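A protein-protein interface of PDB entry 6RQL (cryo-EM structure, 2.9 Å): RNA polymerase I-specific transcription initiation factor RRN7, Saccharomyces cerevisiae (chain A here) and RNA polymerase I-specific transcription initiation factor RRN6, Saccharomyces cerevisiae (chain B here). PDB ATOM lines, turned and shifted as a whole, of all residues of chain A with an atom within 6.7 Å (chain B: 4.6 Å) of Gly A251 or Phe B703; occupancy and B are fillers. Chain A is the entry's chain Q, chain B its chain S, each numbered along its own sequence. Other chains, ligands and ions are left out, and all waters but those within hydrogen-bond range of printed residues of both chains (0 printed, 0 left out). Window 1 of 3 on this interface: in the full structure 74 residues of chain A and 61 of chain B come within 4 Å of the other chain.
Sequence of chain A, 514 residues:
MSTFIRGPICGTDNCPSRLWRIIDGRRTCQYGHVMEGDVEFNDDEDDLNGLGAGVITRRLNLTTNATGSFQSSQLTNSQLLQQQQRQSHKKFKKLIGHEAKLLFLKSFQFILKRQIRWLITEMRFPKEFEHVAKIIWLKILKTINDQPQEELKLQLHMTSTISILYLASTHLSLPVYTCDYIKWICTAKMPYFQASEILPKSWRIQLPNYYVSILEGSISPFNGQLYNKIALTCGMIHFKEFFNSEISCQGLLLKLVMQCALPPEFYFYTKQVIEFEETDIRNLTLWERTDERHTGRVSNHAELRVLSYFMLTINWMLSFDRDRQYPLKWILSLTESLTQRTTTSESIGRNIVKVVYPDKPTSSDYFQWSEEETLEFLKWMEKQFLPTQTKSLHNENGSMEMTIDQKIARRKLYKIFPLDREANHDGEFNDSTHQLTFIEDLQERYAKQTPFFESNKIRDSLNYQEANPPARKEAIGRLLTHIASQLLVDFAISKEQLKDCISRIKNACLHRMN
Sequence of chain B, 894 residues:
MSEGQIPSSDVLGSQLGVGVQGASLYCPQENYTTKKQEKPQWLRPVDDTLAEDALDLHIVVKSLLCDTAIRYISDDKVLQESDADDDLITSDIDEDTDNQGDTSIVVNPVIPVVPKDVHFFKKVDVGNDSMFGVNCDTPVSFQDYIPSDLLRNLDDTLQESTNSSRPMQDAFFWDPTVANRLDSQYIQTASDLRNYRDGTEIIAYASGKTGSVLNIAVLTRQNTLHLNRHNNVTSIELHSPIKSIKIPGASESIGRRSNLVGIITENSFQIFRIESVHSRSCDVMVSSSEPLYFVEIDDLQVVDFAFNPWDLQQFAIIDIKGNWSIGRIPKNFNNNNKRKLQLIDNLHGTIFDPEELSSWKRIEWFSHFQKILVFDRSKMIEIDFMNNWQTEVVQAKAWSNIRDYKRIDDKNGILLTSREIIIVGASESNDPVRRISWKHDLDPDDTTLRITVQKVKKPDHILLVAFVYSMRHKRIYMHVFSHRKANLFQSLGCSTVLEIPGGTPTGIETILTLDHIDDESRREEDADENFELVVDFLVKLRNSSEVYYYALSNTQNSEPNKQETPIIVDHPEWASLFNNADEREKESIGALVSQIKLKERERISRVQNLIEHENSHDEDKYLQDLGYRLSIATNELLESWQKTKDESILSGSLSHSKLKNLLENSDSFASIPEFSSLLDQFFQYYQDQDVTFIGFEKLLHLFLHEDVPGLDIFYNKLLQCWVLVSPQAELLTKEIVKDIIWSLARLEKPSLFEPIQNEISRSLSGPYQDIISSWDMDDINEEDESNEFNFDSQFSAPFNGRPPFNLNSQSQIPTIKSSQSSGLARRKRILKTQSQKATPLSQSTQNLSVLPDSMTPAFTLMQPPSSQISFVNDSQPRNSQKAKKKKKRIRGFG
Of the printed residues of chain B, Gly A251 touches Phe B703 (3.6 Å) and Ile B740 (3.9 Å). Phe B703 touches just these residues of chain A: Pro A175 (3.6 Å), Gly A251 (3.6 Å), Leu A254 (3.7 Å) and Met A258 (3.4 Å). Of the printed residues of chain A, Ile B740 touches Gly A251 and Leu A254. Of the printed residues of chain B, Phe A438 touches Leu B704 and His B705. Of the printed residues of chain A, Leu B702 touches Pro A175 (3.7 Å). Printed residues of chain A within 4 Å of His B705: Lys A255 (3.9 Å) and Phe A438 (3.5 Å). Val A257 touches none of the printed residues of chain B. Leu B700 touches none of the printed residues of chain A.
Pro A175 touches Phe B703. CE1 of Phe B703 touches CA of Gly A251, 3.6 Å away. Gly A251 touches Ile B740 (CA to CD1, 3.9 Å). Leu A254 touches Phe B703 (CD2 to CE1, 3.7 Å). Leu A254 touches Ile B740. CE of Lys A255 touches NE2 of His B705, at 3.9 Å. Met A258 touches Phe B703. CE of Met A258 touches CD2 of Leu B704 (3.7 Å). CB of Phe A438 touches O of Leu B704, at 3.8 Å. Phe A438 touches His B705 (CD2 to CD2, 3.5 Å).
Along chain A the printed residues that touch a printed residue of chain B span positions 175 to 438.
The side-chain hydroxyl (OH) of Tyr A177 lies close to the backbone NH (N) of Gly A251, at 3.5 Å.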
ATOM      1  N   PRO A 175       1.087 -10.101   9.549  1.00  0.00           N
ATOM      2  CA  PRO A 175       0.977  -9.337   8.300  1.00  0.00           C
ATOM      3  C   PRO A 175       2.183  -9.502   7.388  1.00  0.00           C
ATOM      4  O   PRO A 175       2.398  -8.700   6.477  1.00  0.00           O
ATOM      5  CB  PRO A 175       0.838  -7.894   8.794  1.00  0.00           C
ATOM      6  CG  PRO A 175       1.587  -7.878  10.060  1.00  0.00           C
ATOM      7  CD  PRO A 175       1.391  -9.230  10.696  1.00  0.00           C
ATOM      8  N   TYR A 177       3.918 -11.545   4.364  1.00  0.00           N
ATOM      9  CA  TYR A 177       3.375 -12.229   3.202  1.00  0.00           C
ATOM     10  C   TYR A 177       4.491 -12.985   2.505  1.00  0.00           C
ATOM     11  O   TYR A 177       5.627 -13.028   2.975  1.00  0.00           O
ATOM     12  CB  TYR A 177       2.689 -11.242   2.259  1.00  0.00           C
ATOM     13  CG  TYR A 177       1.536 -10.555   2.931  1.00  0.00           C
ATOM     14  CD1 TYR A 177       0.366 -11.246   3.212  1.00  0.00           C
ATOM     15  CD2 TYR A 177       1.616  -9.224   3.297  1.00  0.00           C
ATOM     16  CE1 TYR A 177      -0.689 -10.628   3.842  1.00  0.00           C
ATOM     17  CE2 TYR A 177       0.565  -8.596   3.924  1.00  0.00           C
ATOM     18  CZ  TYR A 177      -0.579  -9.303   4.204  1.00  0.00           C
ATOM     19  OH  TYR A 177      -1.627  -8.667   4.826  1.00  0.00           O
ATOM     20  N   SER A 248      -4.506 -13.012   6.329  1.00  0.00           N
ATOM     21  CA  SER A 248      -4.673 -11.612   6.693  1.00  0.00           C
ATOM     22  C   SER A 248      -4.542 -10.717   5.468  1.00  0.00           C
ATOM     23  O   SER A 248      -3.522 -10.049   5.283  1.00  0.00           O
ATOM     24  CB  SER A 248      -3.649 -11.230   7.762  1.00  0.00           C
ATOM     25  OG  SER A 248      -2.324 -11.412   7.290  1.00  0.00           O
ATOM     26  N   CYS A 249      -5.584 -10.679   4.644  1.00  0.00           N
ATOM     27  CA  CYS A 249      -5.545 -10.013   3.351  1.00  0.00           C
ATOM     28  C   CYS A 249      -5.759  -8.513   3.447  1.00  0.00           C
ATOM     29  O   CYS A 249      -5.678  -7.820   2.431  1.00  0.00           O
ATOM     30  CB  CYS A 249      -6.598 -10.620   2.425  1.00  0.00           C
ATOM     31  SG  CYS A 249      -6.324 -12.363   2.084  1.00  0.00           S
ATOM     32  N   GLN A 250      -6.027  -7.998   4.637  1.00  0.00           N
ATOM     33  CA  GLN A 250      -6.324  -6.585   4.779  1.00  0.00           C
ATOM     34  C   GLN A 250      -5.071  -5.735   4.777  1.00  0.00           C
ATOM     35  O   GLN A 250      -5.073  -4.656   4.180  1.00  0.00           O
ATOM     36  CB  GLN A 250      -7.129  -6.339   6.061  1.00  0.00           C
ATOM     37  CG  GLN A 250      -8.556  -6.885   6.024  1.00  0.00           C
ATOM     38  CD  GLN A 250      -8.632  -8.373   6.302  1.00  0.00           C
ATOM     39  OE1 GLN A 250      -7.675  -8.968   6.792  1.00  0.00           O
ATOM     40  NE2 GLN A 250      -9.765  -8.983   5.979  1.00  0.00           N
ATOM     41  N   GLY A 251      -3.993  -6.211   5.390  1.00  0.00           N
ATOM     42  CA  GLY A 251      -2.726  -5.517   5.313  1.00  0.00           C
ATOM     43  C   GLY A 251      -2.086  -5.667   3.950  1.00  0.00           C
ATOM     44  O   GLY A 251      -1.304  -4.808   3.527  1.00  0.00           O
ATOM     45  N   LEU A 252      -2.408  -6.768   3.262  1.00  0.00           N
ATOM     46  CA  LEU A 252      -1.946  -6.970   1.897  1.00  0.00           C
ATOM     47  C   LEU A 252      -2.510  -5.902   0.981  1.00  0.00           C
ATOM     48  O   LEU A 252      -1.814  -5.423   0.085  1.00  0.00           O
ATOM     49  CB  LEU A 252      -2.356  -8.356   1.394  1.00  0.00           C
ATOM     50  CG  LEU A 252      -1.585  -9.017   0.243  1.00  0.00           C
ATOM     51  CD1 LEU A 252      -1.743 -10.518   0.349  1.00  0.00           C
ATOM     52  CD2 LEU A 252      -1.974  -8.564  -1.156  1.00  0.00           C
ATOM     53  N   LEU A 253      -3.759  -5.510   1.203  1.00  0.00           N
ATOM     54  CA  LEU A 253      -4.292  -4.356   0.502  1.00  0.00           C
ATOM     55  C   LEU A 253      -3.619  -3.087   0.987  1.00  0.00           C
ATOM     56  O   LEU A 253      -3.304  -2.208   0.182  1.00  0.00           O
ATOM     57  CB  LEU A 253      -5.800  -4.277   0.705  1.00  0.00           C
ATOM     58  CG  LEU A 253      -6.537  -5.503   0.175  1.00  0.00           C
ATOM     59  CD1 LEU A 253      -8.007  -5.424   0.515  1.00  0.00           C
ATOM     60  CD2 LEU A 253      -6.316  -5.601  -1.311  1.00  0.00           C
ATOM     61  N   LEU A 254      -3.359  -2.999   2.298  1.00  0.00           N
ATOM     62  CA  LEU A 254      -2.700  -1.825   2.861  1.00  0.00           C
ATOM     63  C   LEU A 254      -1.261  -1.697   2.391  1.00  0.00           C
ATOM     64  O   LEU A 254      -0.822  -0.589   2.060  1.00  0.00           O
ATOM     65  CB  LEU A 254      -2.739  -1.874   4.384  1.00  0.00           C
ATOM     66  CG  LEU A 254      -1.983  -0.740   5.087  1.00  0.00           C
ATOM     67  CD1 LEU A 254      -2.547   0.616   4.708  1.00  0.00           C
ATOM     68  CD2 LEU A 254      -1.979  -0.916   6.599  1.00  0.00           C
ATOM     69  N   LYS A 255      -0.515  -2.803   2.350  1.00  0.00           N
ATOM     70  CA  LYS A 255       0.856  -2.736   1.858  1.00  0.00           C
ATOM     71  C   LYS A 255       0.888  -2.398   0.370  1.00  0.00           C
ATOM     72  O   LYS A 255       1.695  -1.572  -0.070  1.00  0.00           O
ATOM     73  CB  LYS A 255       1.588  -4.045   2.143  1.00  0.00           C
ATOM     74  CG  LYS A 255       3.053  -3.969   1.803  1.00  0.00           C
ATOM     75  CD  LYS A 255       3.782  -5.247   2.131  1.00  0.00           C
ATOM     76  CE  LYS A 255       5.223  -5.166   1.647  1.00  0.00           C
ATOM     77  NZ  LYS A 255       5.971  -6.437   1.835  1.00  0.00           N
ATOM     78  N   LEU A 256      -0.024  -2.981  -0.412  1.00  0.00           N
ATOM     79  CA  LEU A 256      -0.097  -2.663  -1.833  1.00  0.00           C
ATOM     80  C   LEU A 256      -0.657  -1.271  -2.104  1.00  0.00           C
ATOM     81  O   LEU A 256      -0.525  -0.783  -3.229  1.00  0.00           O
ATOM     82  CB  LEU A 256      -0.909  -3.726  -2.574  1.00  0.00           C
ATOM     83  CG  LEU A 256      -0.130  -4.907  -3.174  1.00  0.00           C
ATOM     84  CD1 LEU A 256       0.536  -5.802  -2.152  1.00  0.00           C
ATOM     85  CD2 LEU A 256      -1.047  -5.747  -4.035  1.00  0.00           C
ATOM     86  N   VAL A 257      -1.290  -0.624  -1.121  1.00  0.00           N
ATOM     87  CA  VAL A 257      -1.461   0.826  -1.201  1.00  0.00           C
ATOM     88  C   VAL A 257      -0.106   1.508  -1.104  1.00  0.00           C
ATOM     89  O   VAL A 257       0.262   2.330  -1.951  1.00  0.00           O
ATOM     90  CB  VAL A 257      -2.414   1.333  -0.100  1.00  0.00           C
ATOM     91  CG1 VAL A 257      -2.357   2.847  -0.002  1.00  0.00           C
ATOM     92  CG2 VAL A 257      -3.843   0.906  -0.367  1.00  0.00           C
ATOM     93  N   MET A 258       0.666   1.149  -0.086  1.00  0.00           N
ATOM     94  CA  MET A 258       1.957   1.759   0.172  1.00  0.00           C
ATOM     95  C   MET A 258       3.026   1.318  -0.816  1.00  0.00           C
ATOM     96  O   MET A 258       4.070   1.970  -0.900  1.00  0.00           O
ATOM     97  CB  MET A 258       2.392   1.407   1.590  1.00  0.00           C
ATOM     98  CG  MET A 258       1.472   1.934   2.665  1.00  0.00           C
ATOM     99  SD  MET A 258       1.855   1.142   4.228  1.00  0.00           S
ATOM    100  CE  MET A 258       3.475   1.815   4.554  1.00  0.00           C
ATOM    101  N   TYR A 267      -8.111   1.255  -1.200  1.00  0.00           N
ATOM    102  CA  TYR A 267      -8.214   0.252  -0.153  1.00  0.00           C
ATOM    103  C   TYR A 267      -9.651  -0.215   0.006  1.00  0.00           C
ATOM    104  O   TYR A 267      -9.901  -1.390   0.297  1.00  0.00           O
ATOM    105  CB  TYR A 267      -7.686   0.810   1.164  1.00  0.00           C
ATOM    106  CG  TYR A 267      -7.703  -0.183   2.287  1.00  0.00           C
ATOM    107  CD1 TYR A 267      -6.751  -1.181   2.353  1.00  0.00           C
ATOM    108  CD2 TYR A 267      -8.665  -0.124   3.280  1.00  0.00           C
ATOM    109  CE1 TYR A 267      -6.747  -2.093   3.379  1.00  0.00           C
ATOM    110  CE2 TYR A 267      -8.669  -1.038   4.317  1.00  0.00           C
ATOM    111  CZ  TYR A 267      -7.702  -2.020   4.357  1.00  0.00           C
ATOM    112  OH  TYR A 267      -7.694  -2.944   5.373  1.00  0.00           O
ATOM    113  N   LYS A 271     -11.888  -3.707  -1.408  1.00  0.00           N
ATOM    114  CA  LYS A 271     -12.478  -4.609  -0.435  1.00  0.00           C
ATOM    115  C   LYS A 271     -13.981  -4.739  -0.642  1.00  0.00           C
ATOM    116  O   LYS A 271     -14.588  -5.706  -0.174  1.00  0.00           O
ATOM    117  CB  LYS A 271     -12.132  -4.133   0.971  1.00  0.00           C
ATOM    118  CG  LYS A 271     -12.324  -5.175   2.039  1.00  0.00           C
ATOM    119  CD  LYS A 271     -11.904  -4.639   3.370  1.00  0.00           C
ATOM    120  CE  LYS A 271     -10.404  -4.554   3.441  1.00  0.00           C
ATOM    121  NZ  LYS A 271      -9.989  -4.132   4.785  1.00  0.00           N
ATOM    122  N   PHE A 438      11.431   4.006   4.154  1.00  0.00           N
ATOM    123  CA  PHE A 438      10.307   3.697   3.278  1.00  0.00           C
ATOM    124  C   PHE A 438       9.183   4.723   3.389  1.00  0.00           C
ATOM    125  O   PHE A 438       8.333   4.812   2.496  1.00  0.00           O
ATOM    126  CB  PHE A 438       9.793   2.290   3.602  1.00  0.00           C
ATOM    127  CG  PHE A 438       8.679   1.831   2.714  1.00  0.00           C
ATOM    128  CD1 PHE A 438       8.925   1.487   1.394  1.00  0.00           C
ATOM    129  CD2 PHE A 438       7.386   1.754   3.193  1.00  0.00           C
ATOM    130  CE1 PHE A 438       7.898   1.074   0.572  1.00  0.00           C
ATOM    131  CE2 PHE A 438       6.355   1.337   2.374  1.00  0.00           C
ATOM    132  CZ  PHE A 438       6.614   0.997   1.064  1.00  0.00           C
ATOM    133  N   LEU B 700       4.069  -4.267  14.648  1.00  0.00           N
ATOM    134  CA  LEU B 700       3.486  -3.364  13.671  1.00  0.00           C
ATOM    135  C   LEU B 700       4.551  -2.711  12.798  1.00  0.00           C
ATOM    136  O   LEU B 700       4.218  -1.930  11.902  1.00  0.00           O
ATOM    137  CB  LEU B 700       2.650  -2.309  14.400  1.00  0.00           C
ATOM    138  CG  LEU B 700       1.630  -1.377  13.746  1.00  0.00           C
ATOM    139  CD1 LEU B 700       0.472  -2.172  13.183  1.00  0.00           C
ATOM    140  CD2 LEU B 700       1.139  -0.378  14.761  1.00  0.00           C
ATOM    141  N   HIS B 701       5.823  -3.046  13.008  1.00  0.00           N
ATOM    142  CA  HIS B 701       6.905  -2.507  12.194  1.00  0.00           C
ATOM    143  C   HIS B 701       6.983  -3.157  10.819  1.00  0.00           C
ATOM    144  O   HIS B 701       7.763  -2.700   9.979  1.00  0.00           O
ATOM    145  CB  HIS B 701       8.248  -2.683  12.904  1.00  0.00           C
ATOM    146  CG  HIS B 701       8.724  -4.098  12.939  1.00  0.00           C
ATOM    147  ND1 HIS B 701       9.546  -4.633  11.971  1.00  0.00           N
ATOM    148  CD2 HIS B 701       8.467  -5.103  13.808  1.00  0.00           C
ATOM    149  CE1 HIS B 701       9.789  -5.900  12.252  1.00  0.00           C
ATOM    150  NE2 HIS B 701       9.144  -6.211  13.361  1.00  0.00           N
ATOM    151  N   LEU B 702       6.200  -4.205  10.571  1.00  0.00           N
ATOM    152  CA  LEU B 702       6.218  -4.889   9.286  1.00  0.00           C
ATOM    153  C   LEU B 702       5.570  -4.077   8.170  1.00  0.00           C
ATOM    154  O   LEU B 702       5.741  -4.424   6.997  1.00  0.00           O
ATOM    155  CB  LEU B 702       5.511  -6.242   9.404  1.00  0.00           C
ATOM    156  CG  LEU B 702       6.095  -7.254  10.392  1.00  0.00           C
ATOM    157  CD1 LEU B 702       5.257  -8.524  10.411  1.00  0.00           C
ATOM    158  CD2 LEU B 702       7.541  -7.578  10.077  1.00  0.00           C
ATOM    159  N   PHE B 703       4.837  -3.015   8.499  1.00  0.00           N
ATOM    160  CA  PHE B 703       4.190  -2.168   7.508  1.00  0.00           C
ATOM    161  C   PHE B 703       5.059  -0.994   7.084  1.00  0.00           C
ATOM    162  O   PHE B 703       5.287  -0.792   5.889  1.00  0.00           O
ATOM    163  CB  PHE B 703       2.860  -1.639   8.049  1.00  0.00           C
ATOM    164  CG  PHE B 703       1.782  -2.666   8.119  1.00  0.00           C
ATOM    165  CD1 PHE B 703       1.048  -2.986   6.994  1.00  0.00           C
ATOM    166  CD2 PHE B 703       1.493  -3.307   9.310  1.00  0.00           C
ATOM    167  CE1 PHE B 703       0.051  -3.925   7.048  1.00  0.00           C
ATOM    168  CE2 PHE B 703       0.494  -4.250   9.369  1.00  0.00           C
ATOM    169  CZ  PHE B 703      -0.230  -4.555   8.230  1.00  0.00           C
ATOM    170  N   LEU B 704       5.548  -0.214   8.040  1.00  0.00           N
ATOM    171  CA  LEU B 704       6.284   0.997   7.723  1.00  0.00           C
ATOM    172  C   LEU B 704       7.749   0.756   7.414  1.00  0.00           C
ATOM    173  O   LEU B 704       8.441   1.719   7.059  1.00  0.00           O
ATOM    174  CB  LEU B 704       6.167   2.001   8.868  1.00  0.00           C
ATOM    175  CG  LEU B 704       4.801   2.671   8.922  1.00  0.00           C
ATOM    176  CD1 LEU B 704       4.652   3.551  10.145  1.00  0.00           C
ATOM    177  CD2 LEU B 704       4.653   3.489   7.662  1.00  0.00           C
ATOM    178  N   HIS B 705       8.224  -0.490   7.558  1.00  0.00           N
ATOM    179  CA  HIS B 705       9.589  -0.904   7.216  1.00  0.00           C
ATOM    180  C   HIS B 705      10.636  -0.096   7.978  1.00  0.00           C
ATOM    181  O   HIS B 705      11.719   0.192   7.467  1.00  0.00           O
ATOM    182  CB  HIS B 705       9.832  -0.831   5.708  1.00  0.00           C
ATOM    183  CG  HIS B 705       8.999  -1.789   4.917  1.00  0.00           C
ATOM    184  ND1 HIS B 705       9.293  -3.132   4.827  1.00  0.00           N
ATOM    185  CD2 HIS B 705       7.878  -1.599   4.184  1.00  0.00           C
ATOM    186  CE1 HIS B 705       8.392  -3.727   4.068  1.00  0.00           C
ATOM    187  NE2 HIS B 705       7.521  -2.820   3.666  1.00  0.00           N
ATOM    188  N   PHE B 714       2.312   5.413  14.534  1.00  0.00           N
ATOM    189  CA  PHE B 714       1.930   4.649  13.357  1.00  0.00           C
ATOM    190  C   PHE B 714       0.869   5.399  12.571  1.00  0.00           C
ATOM    191  O   PHE B 714       0.993   5.575  11.356  1.00  0.00           O
ATOM    192  CB  PHE B 714       1.416   3.280  13.782  1.00  0.00           C
ATOM    193  CG  PHE B 714       0.883   2.441  12.662  1.00  0.00           C
ATOM    194  CD1 PHE B 714       1.739   1.751  11.828  1.00  0.00           C
ATOM    195  CD2 PHE B 714      -0.484   2.316  12.468  1.00  0.00           C
ATOM    196  CE1 PHE B 714       1.242   0.963  10.816  1.00  0.00           C
ATOM    197  CE2 PHE B 714      -0.985   1.539  11.459  1.00  0.00           C
ATOM    198  CZ  PHE B 714      -0.124   0.862  10.630  1.00  0.00           C
ATOM    199  N   ILE B 740      -7.371  -2.790  10.321  1.00  0.00           N
ATOM    200  CA  ILE B 740      -6.184  -3.602  10.572  1.00  0.00           C
ATOM    201  C   ILE B 740      -6.276  -4.294  11.926  1.00  0.00           C
ATOM    202  O   ILE B 740      -6.028  -5.501  12.032  1.00  0.00           O
ATOM    203  CB  ILE B 740      -4.910  -2.747  10.454  1.00  0.00           C
ATOM    204  CG1 ILE B 740      -4.698  -2.295   9.012  1.00  0.00           C
ATOM    205  CG2 ILE B 740      -3.685  -3.508  10.949  1.00  0.00           C
ATOM    206  CD1 ILE B 740      -4.504  -3.435   8.047  1.00  0.00           C
